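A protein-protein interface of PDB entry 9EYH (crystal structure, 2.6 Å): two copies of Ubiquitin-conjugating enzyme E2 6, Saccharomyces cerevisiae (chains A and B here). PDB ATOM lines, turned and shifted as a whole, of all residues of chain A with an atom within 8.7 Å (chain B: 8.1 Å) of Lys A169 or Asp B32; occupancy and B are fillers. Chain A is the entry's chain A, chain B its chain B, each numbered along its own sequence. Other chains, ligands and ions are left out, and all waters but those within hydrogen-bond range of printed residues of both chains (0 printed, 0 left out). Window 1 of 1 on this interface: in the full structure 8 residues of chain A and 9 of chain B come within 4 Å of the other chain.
The side-chain amide nitrogen (ND2) of Asn A138 lies close to the side-chain amide nitrogen (ND2) of Asn B33, at 3.5 Å. The side-chain carboxylate (OD2) of Asp B32 is in salt-bridge range of the side-chain amino group (NZ) of Lys A169 (3.2 Å). The side-chain amino group (NZ) of Lys A169 lies within salt-bridge range of the side-chain carboxylate (OE2) of Glu B31 (3.3 Å). The guanidinium group (NH2) of Arg A137 lies within salt-bridge range of the side-chain carboxylate (OD1) of Asp B32.
The backbone NH (N) of Asp B32 lies close to the side-chain amide oxygen (OD1) of Asn B30 (3.3 Å). O of Thr A134 is in hydrogen-bond range of ND2 of Asn A138 (3.1 Å). The side-chain amide oxygen of Asn B33 lies close to the backbone NH of Leu B35 (3.2 Å).
O of Asp B32 touches OD1 of Asn A138 (3.8 Å). Val A162 touches Val B148. Leu B152 touches Glu A166. CG of Lys A169 touches O of Leu B152 (3.6 Å).
Of chain B, only Glu B31 (3.3 Å), Asp B32 (3.2 Å) and Leu B152 (3.6 Å) come within 4 Å of Lys A169. Asp B32 touches just these residues of chain A: Arg A137, Asn A138 and Lys A169. Of the printed residues of chain B, Val A162 touches Val B148 (3.97 Å). Printed residues of chain A within 4 Å of Glu B31: Lys A169 (3.3 Å). Printed residues of chain A within 4 Å of Leu B152: Glu A166 (3.8 Å) and Lys A169 (3.6 Å). Printed residues of chain B within 4 Å of Asn A138: Asp B32 (3.8 Å) and Asn B33 (3.5 Å). Pro B155 touches none of the printed residues of chain A. The nearest residue of chain B that does not touch Lys A169 is Asn B30 (4.3 Å).
Of the 15 printed residues of chain A, 5 touch a printed residue of chain B. Hydrophobic or aromatic side chains of chain A that line the printed part of chain B: Val A162. Of the 15 printed residues of chain B, 5 touch a printed residue of chain A. Hydrophobic or aromatic side chains of chain B that line the printed part of chain A: Val B148 and Leu B152. Among the printed residues, Asp or Glu carboxylates within 4 Å of a Lys or Arg side-chain nitrogen of the other chain: Arg A137 with Asp B32, Lys A169 with Glu B31 and Lys A169 with Asp B32.
No position is printed for both chains.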
ATOM      1  N   LYS A 133     -30.153 -27.116 -14.411  1.00  0.00           N
ATOM      2  CA  LYS A 133     -30.749 -26.187 -13.457  1.00  0.00           C
ATOM      3  C   LYS A 133     -29.748 -25.135 -12.996  1.00  0.00           C
ATOM      4  O   LYS A 133     -30.144 -24.008 -12.676  1.00  0.00           O
ATOM      5  CB  LYS A 133     -31.316 -26.951 -12.260  1.00  0.00           C
ATOM      6  CG  LYS A 133     -32.548 -27.777 -12.596  1.00  0.00           C
ATOM      7  CD  LYS A 133     -32.997 -28.632 -11.426  1.00  0.00           C
ATOM      8  CE  LYS A 133     -34.285 -29.370 -11.760  1.00  0.00           C
ATOM      9  NZ  LYS A 133     -34.629 -30.389 -10.730  1.00  0.00           N
ATOM     10  N   THR A 134     -28.458 -25.476 -12.958  1.00  0.00           N
ATOM     11  CA  THR A 134     -27.442 -24.483 -12.619  1.00  0.00           C
ATOM     12  C   THR A 134     -27.375 -23.392 -13.680  1.00  0.00           C
ATOM     13  O   THR A 134     -27.341 -22.197 -13.363  1.00  0.00           O
ATOM     14  CB  THR A 134     -26.078 -25.157 -12.457  1.00  0.00           C
ATOM     15  OG1 THR A 134     -26.215 -26.330 -11.648  1.00  0.00           O
ATOM     16  CG2 THR A 134     -25.095 -24.208 -11.793  1.00  0.00           C
ATOM     17  N   LEU A 135     -27.358 -23.789 -14.954  1.00  0.00           N
ATOM     18  CA  LEU A 135     -27.301 -22.813 -16.036  1.00  0.00           C
ATOM     19  C   LEU A 135     -28.592 -22.011 -16.139  1.00  0.00           C
ATOM     20  O   LEU A 135     -28.566 -20.854 -16.572  1.00  0.00           O
ATOM     21  CB  LEU A 135     -26.999 -23.519 -17.357  1.00  0.00           C
ATOM     22  CG  LEU A 135     -25.680 -24.296 -17.381  1.00  0.00           C
ATOM     23  CD1 LEU A 135     -25.677 -25.321 -18.500  1.00  0.00           C
ATOM     24  CD2 LEU A 135     -24.498 -23.349 -17.519  1.00  0.00           C
ATOM     25  N   ARG A 137     -30.356 -20.953 -13.581  1.00  0.00           N
ATOM     26  CA  ARG A 137     -30.237 -19.889 -12.589  1.00  0.00           C
ATOM     27  C   ARG A 137     -29.248 -18.821 -13.036  1.00  0.00           C
ATOM     28  O   ARG A 137     -29.475 -17.626 -12.815  1.00  0.00           O
ATOM     29  CB  ARG A 137     -29.818 -20.470 -11.239  1.00  0.00           C
ATOM     30  CG  ARG A 137     -30.973 -20.894 -10.352  1.00  0.00           C
ATOM     31  CD  ARG A 137     -30.536 -20.939  -8.899  1.00  0.00           C
ATOM     32  NE  ARG A 137     -29.758 -19.756  -8.546  1.00  0.00           N
ATOM     33  CZ  ARG A 137     -30.281 -18.589  -8.198  1.00  0.00           C
ATOM     34  NH1 ARG A 137     -31.590 -18.411  -8.126  1.00  0.00           N
ATOM     35  NH2 ARG A 137     -29.471 -17.572  -7.917  1.00  0.00           N
ATOM     36  N   ASN A 138     -28.147 -19.229 -13.665  1.00  0.00           N
ATOM     37  CA  ASN A 138     -27.118 -18.288 -14.087  1.00  0.00           C
ATOM     38  C   ASN A 138     -27.437 -17.598 -15.405  1.00  0.00           C
ATOM     39  O   ASN A 138     -26.686 -16.705 -15.811  1.00  0.00           O
ATOM     40  CB  ASN A 138     -25.770 -19.004 -14.209  1.00  0.00           C
ATOM     41  CG  ASN A 138     -25.347 -19.673 -12.918  1.00  0.00           C
ATOM     42  OD1 ASN A 138     -25.712 -19.234 -11.827  1.00  0.00           O
ATOM     43  ND2 ASN A 138     -24.570 -20.744 -13.036  1.00  0.00           N
ATOM     44  N   SER A 141     -27.948 -13.706 -15.239  1.00  0.00           N
ATOM     45  CA  SER A 141     -26.689 -12.995 -15.044  1.00  0.00           C
ATOM     46  C   SER A 141     -25.814 -13.046 -16.292  1.00  0.00           C
ATOM     47  O   SER A 141     -25.050 -12.109 -16.547  1.00  0.00           O
ATOM     48  CB  SER A 141     -25.938 -13.573 -13.845  1.00  0.00           C
ATOM     49  OG  SER A 141     -24.719 -12.883 -13.629  1.00  0.00           O
ATOM     50  N   VAL A 162     -31.452  -6.554 -14.231  1.00  0.00           N
ATOM     51  CA  VAL A 162     -30.755  -5.903 -13.126  1.00  0.00           C
ATOM     52  C   VAL A 162     -31.696  -5.714 -11.944  1.00  0.00           C
ATOM     53  O   VAL A 162     -31.321  -5.945 -10.788  1.00  0.00           O
ATOM     54  CB  VAL A 162     -30.147  -4.565 -13.588  1.00  0.00           C
ATOM     55  CG1 VAL A 162     -29.579  -3.799 -12.403  1.00  0.00           C
ATOM     56  CG2 VAL A 162     -29.065  -4.804 -14.632  1.00  0.00           C
ATOM     57  N   GLU A 163     -32.937  -5.298 -12.215  1.00  0.00           N
ATOM     58  CA  GLU A 163     -33.929  -5.190 -11.151  1.00  0.00           C
ATOM     59  C   GLU A 163     -34.212  -6.547 -10.520  1.00  0.00           C
ATOM     60  O   GLU A 163     -34.346  -6.654  -9.296  1.00  0.00           O
ATOM     61  CB  GLU A 163     -35.220  -4.579 -11.696  1.00  0.00           C
ATOM     62  CG  GLU A 163     -35.058  -3.172 -12.239  1.00  0.00           C
ATOM     63  CD  GLU A 163     -36.318  -2.655 -12.900  1.00  0.00           C
ATOM     64  OE1 GLU A 163     -37.337  -3.379 -12.900  1.00  0.00           O
ATOM     65  OE2 GLU A 163     -36.290  -1.520 -13.421  1.00  0.00           O
ATOM     66  N   THR A 164     -34.301  -7.596 -11.342  1.00  0.00           N
ATOM     67  CA  THR A 164     -34.553  -8.933 -10.814  1.00  0.00           C
ATOM     68  C   THR A 164     -33.407  -9.398  -9.919  1.00  0.00           C
ATOM     69  O   THR A 164     -33.639  -9.963  -8.843  1.00  0.00           O
ATOM     70  CB  THR A 164     -34.772  -9.922 -11.962  1.00  0.00           C
ATOM     71  OG1 THR A 164     -35.762  -9.407 -12.863  1.00  0.00           O
ATOM     72  CG2 THR A 164     -35.239 -11.266 -11.425  1.00  0.00           C
ATOM     73  N   LEU A 165     -32.164  -9.156 -10.342  1.00  0.00           N
ATOM     74  CA  LEU A 165     -31.014  -9.612  -9.568  1.00  0.00           C
ATOM     75  C   LEU A 165     -30.857  -8.820  -8.275  1.00  0.00           C
ATOM     76  O   LEU A 165     -30.521  -9.391  -7.232  1.00  0.00           O
ATOM     77  CB  LEU A 165     -29.744  -9.515 -10.411  1.00  0.00           C
ATOM     78  CG  LEU A 165     -29.694 -10.428 -11.635  1.00  0.00           C
ATOM     79  CD1 LEU A 165     -28.474 -10.115 -12.483  1.00  0.00           C
ATOM     80  CD2 LEU A 165     -29.695 -11.888 -11.209  1.00  0.00           C
ATOM     81  N   GLU A 166     -31.083  -7.505  -8.325  1.00  0.00           N
ATOM     82  CA  GLU A 166     -30.977  -6.689  -7.119  1.00  0.00           C
ATOM     83  C   GLU A 166     -31.945  -7.170  -6.045  1.00  0.00           C
ATOM     84  O   GLU A 166     -31.565  -7.328  -4.878  1.00  0.00           O
ATOM     85  CB  GLU A 166     -31.232  -5.220  -7.452  1.00  0.00           C
ATOM     86  CG  GLU A 166     -30.094  -4.544  -8.193  1.00  0.00           C
ATOM     87  CD  GLU A 166     -30.461  -3.154  -8.663  1.00  0.00           C
ATOM     88  OE1 GLU A 166     -31.670  -2.867  -8.775  1.00  0.00           O
ATOM     89  OE2 GLU A 166     -29.542  -2.346  -8.917  1.00  0.00           O
ATOM     90  N   LYS A 167     -33.201  -7.418  -6.426  1.00  0.00           N
ATOM     91  CA  LYS A 167     -34.210  -7.847  -5.460  1.00  0.00           C
ATOM     92  C   LYS A 167     -33.873  -9.210  -4.868  1.00  0.00           C
ATOM     93  O   LYS A 167     -34.129  -9.463  -3.685  1.00  0.00           O
ATOM     94  CB  LYS A 167     -35.586  -7.873  -6.127  1.00  0.00           C
ATOM     95  CG  LYS A 167     -36.074  -6.508  -6.580  1.00  0.00           C
ATOM     96  CD  LYS A 167     -37.164  -6.631  -7.627  1.00  0.00           C
ATOM     97  CE  LYS A 167     -38.387  -7.332  -7.072  1.00  0.00           C
ATOM     98  NZ  LYS A 167     -39.463  -7.416  -8.094  1.00  0.00           N
ATOM     99  N   ARG A 168     -33.297 -10.102  -5.678  1.00  0.00           N
ATOM    100  CA  ARG A 168     -32.863 -11.402  -5.175  1.00  0.00           C
ATOM    101  C   ARG A 168     -31.753 -11.271  -4.138  1.00  0.00           C
ATOM    102  O   ARG A 168     -31.623 -12.138  -3.266  1.00  0.00           O
ATOM    103  CB  ARG A 168     -32.408 -12.287  -6.338  1.00  0.00           C
ATOM    104  CG  ARG A 168     -33.558 -12.852  -7.149  1.00  0.00           C
ATOM    105  CD  ARG A 168     -33.145 -13.199  -8.566  1.00  0.00           C
ATOM    106  NE  ARG A 168     -31.980 -14.072  -8.617  1.00  0.00           N
ATOM    107  CZ  ARG A 168     -31.540 -14.659  -9.723  1.00  0.00           C
ATOM    108  NH1 ARG A 168     -32.175 -14.523 -10.876  1.00  0.00           N
ATOM    109  NH2 ARG A 168     -30.438 -15.399  -9.670  1.00  0.00           N
ATOM    110  N   LYS A 169     -30.956 -10.200  -4.209  1.00  0.00           N
ATOM    111  CA  LYS A 169     -29.899  -9.918  -3.242  1.00  0.00           C
ATOM    112  C   LYS A 169     -30.392  -9.068  -2.072  1.00  0.00           C
ATOM    113  O   LYS A 169     -29.592  -8.379  -1.424  1.00  0.00           O
ATOM    114  CB  LYS A 169     -28.721  -9.231  -3.945  1.00  0.00           C
ATOM    115  CG  LYS A 169     -27.379  -9.341  -3.220  1.00  0.00           C
ATOM    116  CD  LYS A 169     -26.972 -10.786  -2.998  1.00  0.00           C
ATOM    117  CE  LYS A 169     -26.673 -11.477  -4.313  1.00  0.00           C
ATOM    118  NZ  LYS A 169     -26.216 -12.875  -4.103  1.00  0.00           N
ATOM    119  N   LEU A 170     -31.691  -9.091  -1.789  1.00  0.00           N
ATOM    120  CA  LEU A 170     -32.253  -8.319  -0.689  1.00  0.00           C
ATOM    121  C   LEU A 170     -33.116  -9.204   0.205  1.00  0.00           C
ATOM    122  O   LEU A 170     -33.733  -8.728   1.157  1.00  0.00           O
ATOM    123  CB  LEU A 170     -33.075  -7.144  -1.218  1.00  0.00           C
ATOM    124  CG  LEU A 170     -32.344  -6.131  -2.102  1.00  0.00           C
ATOM    125  CD1 LEU A 170     -33.311  -5.071  -2.599  1.00  0.00           C
ATOM    126  CD2 LEU A 170     -31.167  -5.493  -1.373  1.00  0.00           C
ATOM    127  N   PRO B  29     -16.263 -16.371  -3.849  1.00  0.00           N
ATOM    128  CA  PRO B  29     -17.162 -16.833  -4.908  1.00  0.00           C
ATOM    129  C   PRO B  29     -18.553 -16.233  -4.776  1.00  0.00           C
ATOM    130  O   PRO B  29     -19.012 -15.887  -3.685  1.00  0.00           O
ATOM    131  CB  PRO B  29     -17.199 -18.350  -4.693  1.00  0.00           C
ATOM    132  CG  PRO B  29     -17.019 -18.497  -3.224  1.00  0.00           C
ATOM    133  CD  PRO B  29     -16.072 -17.396  -2.806  1.00  0.00           C
ATOM    134  N   ASN B  30     -19.220 -16.113  -5.920  1.00  0.00           N
ATOM    135  CA  ASN B  30     -20.613 -15.690  -5.937  1.00  0.00           C
ATOM    136  C   ASN B  30     -21.460 -16.697  -5.171  1.00  0.00           C
ATOM    137  O   ASN B  30     -21.447 -17.893  -5.479  1.00  0.00           O
ATOM    138  CB  ASN B  30     -21.101 -15.556  -7.380  1.00  0.00           C
ATOM    139  CG  ASN B  30     -22.521 -15.029  -7.476  1.00  0.00           C
ATOM    140  OD1 ASN B  30     -23.093 -14.559  -6.493  1.00  0.00           O
ATOM    141  ND2 ASN B  30     -23.094 -15.098  -8.672  1.00  0.00           N
ATOM    142  N   GLU B  31     -22.190 -16.214  -4.161  1.00  0.00           N
ATOM    143  CA  GLU B  31     -22.981 -17.109  -3.322  1.00  0.00           C
ATOM    144  C   GLU B  31     -24.032 -17.875  -4.114  1.00  0.00           C
ATOM    145  O   GLU B  31     -24.504 -18.918  -3.647  1.00  0.00           O
ATOM    146  CB  GLU B  31     -23.645 -16.322  -2.187  1.00  0.00           C
ATOM    147  CG  GLU B  31     -24.132 -14.931  -2.571  1.00  0.00           C
ATOM    148  CD  GLU B  31     -23.072 -13.859  -2.370  1.00  0.00           C
ATOM    149  OE1 GLU B  31     -21.890 -14.215  -2.178  1.00  0.00           O
ATOM    150  OE2 GLU B  31     -23.424 -12.660  -2.400  1.00  0.00           O
ATOM    151  N   ASP B  32     -24.401 -17.395  -5.298  1.00  0.00           N
ATOM    152  CA  ASP B  32     -25.330 -18.096  -6.172  1.00  0.00           C
ATOM    153  C   ASP B  32     -24.630 -18.901  -7.258  1.00  0.00           C
ATOM    154  O   ASP B  32     -25.305 -19.572  -8.045  1.00  0.00           O
ATOM    155  CB  ASP B  32     -26.301 -17.099  -6.811  1.00  0.00           C
ATOM    156  CG  ASP B  32     -27.404 -16.676  -5.864  1.00  0.00           C
ATOM    157  OD1 ASP B  32     -28.225 -17.540  -5.487  1.00  0.00           O
ATOM    158  OD2 ASP B  32     -27.444 -15.486  -5.487  1.00  0.00           O
ATOM    159  N   ASN B  33     -23.300 -18.856  -7.317  1.00  0.00           N
ATOM    160  CA  ASN B  33     -22.557 -19.583  -8.345  1.00  0.00           C
ATOM    161  C   ASN B  33     -21.114 -19.720  -7.879  1.00  0.00           C
ATOM    162  O   ASN B  33     -20.359 -18.742  -7.912  1.00  0.00           O
ATOM    163  CB  ASN B  33     -22.639 -18.861  -9.686  1.00  0.00           C
ATOM    164  CG  ASN B  33     -21.986 -19.640 -10.808  1.00  0.00           C
ATOM    165  OD1 ASN B  33     -21.663 -20.819 -10.658  1.00  0.00           O
ATOM    166  ND2 ASN B  33     -21.795 -18.986 -11.948  1.00  0.00           N
ATOM    167  N   ILE B  34     -20.734 -20.928  -7.454  1.00  0.00           N
ATOM    168  CA  ILE B  34     -19.382 -21.166  -6.965  1.00  0.00           C
ATOM    169  C   ILE B  34     -18.345 -21.024  -8.075  1.00  0.00           C
ATOM    170  O   ILE B  34     -17.170 -20.761  -7.791  1.00  0.00           O
ATOM    171  CB  ILE B  34     -19.300 -22.559  -6.309  1.00  0.00           C
ATOM    172  CG1 ILE B  34     -18.022 -22.701  -5.478  1.00  0.00           C
ATOM    173  CG2 ILE B  34     -19.385 -23.658  -7.358  1.00  0.00           C
ATOM    174  CD1 ILE B  34     -18.141 -22.152  -4.075  1.00  0.00           C
ATOM    175  N   LEU B  35     -18.750 -21.179  -9.338  1.00  0.00           N
ATOM    176  CA  LEU B  35     -17.818 -21.090 -10.457  1.00  0.00           C
ATOM    177  C   LEU B  35     -17.400 -19.659 -10.767  1.00  0.00           C
ATOM    178  O   LEU B  35     -16.366 -19.458 -11.415  1.00  0.00           O
ATOM    179  CB  LEU B  35     -18.443 -21.715 -11.708  1.00  0.00           C
ATOM    180  CG  LEU B  35     -18.760 -23.210 -11.633  1.00  0.00           C
ATOM    181  CD1 LEU B  35     -19.775 -23.590 -12.696  1.00  0.00           C
ATOM    182  CD2 LEU B  35     -17.491 -24.038 -11.781  1.00  0.00           C
ATOM    183  N   GLU B  36     -18.171 -18.669 -10.324  1.00  0.00           N
ATOM    184  CA  GLU B  36     -17.910 -17.261 -10.618  1.00  0.00           C
ATOM    185  C   GLU B  36     -17.365 -16.587  -9.363  1.00  0.00           C
ATOM    186  O   GLU B  36     -18.114 -16.313  -8.420  1.00  0.00           O
ATOM    187  CB  GLU B  36     -19.179 -16.566 -11.109  1.00  0.00           C
ATOM    188  CG  GLU B  36     -19.038 -15.063 -11.272  1.00  0.00           C
ATOM    189  CD  GLU B  36     -20.336 -14.404 -11.692  1.00  0.00           C
ATOM    190  OE1 GLU B  36     -20.935 -14.858 -12.688  1.00  0.00           O
ATOM    191  OE2 GLU B  36     -20.762 -13.443 -11.018  1.00  0.00           O
ATOM    192  N   VAL B 148     -22.796  -2.232 -10.589  1.00  0.00           N
ATOM    193  CA  VAL B 148     -23.927  -2.933  -9.985  1.00  0.00           C
ATOM    194  C   VAL B 148     -23.477  -4.257  -9.378  1.00  0.00           C
ATOM    195  O   VAL B 148     -23.904  -4.630  -8.278  1.00  0.00           O
ATOM    196  CB  VAL B 148     -25.048  -3.127 -11.024  1.00  0.00           C
ATOM    197  CG1 VAL B 148     -24.478  -3.626 -12.344  1.00  0.00           C
ATOM    198  CG2 VAL B 148     -26.108  -4.087 -10.498  1.00  0.00           C
ATOM    199  N   ARG B 149     -22.597  -4.980 -10.076  1.00  0.00           N
ATOM    200  CA  ARG B 149     -22.123  -6.263  -9.565  1.00  0.00           C
ATOM    201  C   ARG B 149     -21.285  -6.096  -8.304  1.00  0.00           C
ATOM    202  O   ARG B 149     -21.238  -7.007  -7.468  1.00  0.00           O
ATOM    203  CB  ARG B 149     -21.325  -6.993 -10.645  1.00  0.00           C
ATOM    204  CG  ARG B 149     -22.182  -7.535 -11.779  1.00  0.00           C
ATOM    205  CD  ARG B 149     -21.334  -8.062 -12.925  1.00  0.00           C
ATOM    206  NE  ARG B 149     -20.701  -6.982 -13.672  1.00  0.00           N
ATOM    207  CZ  ARG B 149     -20.033  -7.144 -14.806  1.00  0.00           C
ATOM    208  NH1 ARG B 149     -19.886  -8.338 -15.356  1.00  0.00           N
ATOM    209  NH2 ARG B 149     -19.501  -6.083 -15.403  1.00  0.00           N
ATOM    210  N   LYS B 151     -21.883  -3.880  -5.856  1.00  0.00           N
ATOM    211  CA  LYS B 151     -22.809  -3.709  -4.742  1.00  0.00           C
ATOM    212  C   LYS B 151     -23.492  -5.020  -4.369  1.00  0.00           C
ATOM    213  O   LYS B 151     -23.809  -5.240  -3.195  1.00  0.00           O
ATOM    214  CB  LYS B 151     -23.841  -2.639  -5.098  1.00  0.00           C
ATOM    215  CG  LYS B 151     -24.829  -2.296  -3.998  1.00  0.00           C
ATOM    216  CD  LYS B 151     -25.783  -1.212  -4.474  1.00  0.00           C
ATOM    217  CE  LYS B 151     -27.178  -1.409  -3.908  1.00  0.00           C
ATOM    218  NZ  LYS B 151     -28.179  -0.569  -4.624  1.00  0.00           N
ATOM    219  N   LEU B 152     -23.719  -5.901  -5.345  1.00  0.00           N
ATOM    220  CA  LEU B 152     -24.354  -7.183  -5.053  1.00  0.00           C
ATOM    221  C   LEU B 152     -23.393  -8.127  -4.341  1.00  0.00           C
ATOM    222  O   LEU B 152     -23.783  -8.829  -3.401  1.00  0.00           O
ATOM    223  CB  LEU B 152     -24.864  -7.823  -6.344  1.00  0.00           C
ATOM    224  CG  LEU B 152     -25.844  -7.020  -7.200  1.00  0.00           C
ATOM    225  CD1 LEU B 152     -26.020  -7.677  -8.561  1.00  0.00           C
ATOM    226  CD2 LEU B 152     -27.184  -6.875  -6.498  1.00  0.00           C
ATOM    227  N   ILE B 153     -22.136  -8.157  -4.773  1.00  0.00           N
ATOM    228  CA  ILE B 153     -21.170  -9.121  -4.254  1.00  0.00           C
ATOM    229  C   ILE B 153     -20.453  -8.591  -3.018  1.00  0.00           C
ATOM    230  O   ILE B 153     -20.211  -9.339  -2.069  1.00  0.00           O
ATOM    231  CB  ILE B 153     -20.175  -9.507  -5.366  1.00  0.00           C
ATOM    232  CG1 ILE B 153     -20.914 -10.163  -6.535  1.00  0.00           C
ATOM    233  CG2 ILE B 153     -19.094 -10.432  -4.828  1.00  0.00           C
ATOM    234  CD1 ILE B 153     -21.774 -11.340  -6.128  1.00  0.00           C
ATOM    235  N   PHE B 154     -20.107  -7.303  -2.998  1.00  0.00           N
ATOM    236  CA  PHE B 154     -19.360  -6.699  -1.897  1.00  0.00           C
ATOM    237  C   PHE B 154     -20.177  -5.568  -1.277  1.00  0.00           C
ATOM    238  O   PHE B 154     -19.872  -4.385  -1.479  1.00  0.00           O
ATOM    239  CB  PHE B 154     -18.002  -6.186  -2.373  1.00  0.00           C
ATOM    240  CG  PHE B 154     -17.182  -7.220  -3.089  1.00  0.00           C
ATOM    241  CD1 PHE B 154     -16.606  -8.269  -2.394  1.00  0.00           C
ATOM    242  CD2 PHE B 154     -16.984  -7.140  -4.457  1.00  0.00           C
ATOM    243  CE1 PHE B 154     -15.850  -9.222  -3.050  1.00  0.00           C
ATOM    244  CE2 PHE B 154     -16.227  -8.090  -5.119  1.00  0.00           C
ATOM    245  CZ  PHE B 154     -15.659  -9.131  -4.414  1.00  0.00           C
ATOM    246  N   PRO B 155     -21.217  -5.898  -0.505  1.00  0.00           N
ATOM    247  CA  PRO B 155     -21.996  -4.827   0.135  1.00  0.00           C
ATOM    248  C   PRO B 155     -21.243  -4.134   1.253  1.00  0.00           C
ATOM    249  O   PRO B 155     -21.377  -2.916   1.423  1.00  0.00           O
ATOM    250  CB  PRO B 155     -23.238  -5.566   0.648  1.00  0.00           C
ATOM    251  CG  PRO B 155     -22.755  -6.952   0.907  1.00  0.00           C
ATOM    252  CD  PRO B 155     -21.721  -7.237  -0.151  1.00  0.00           C
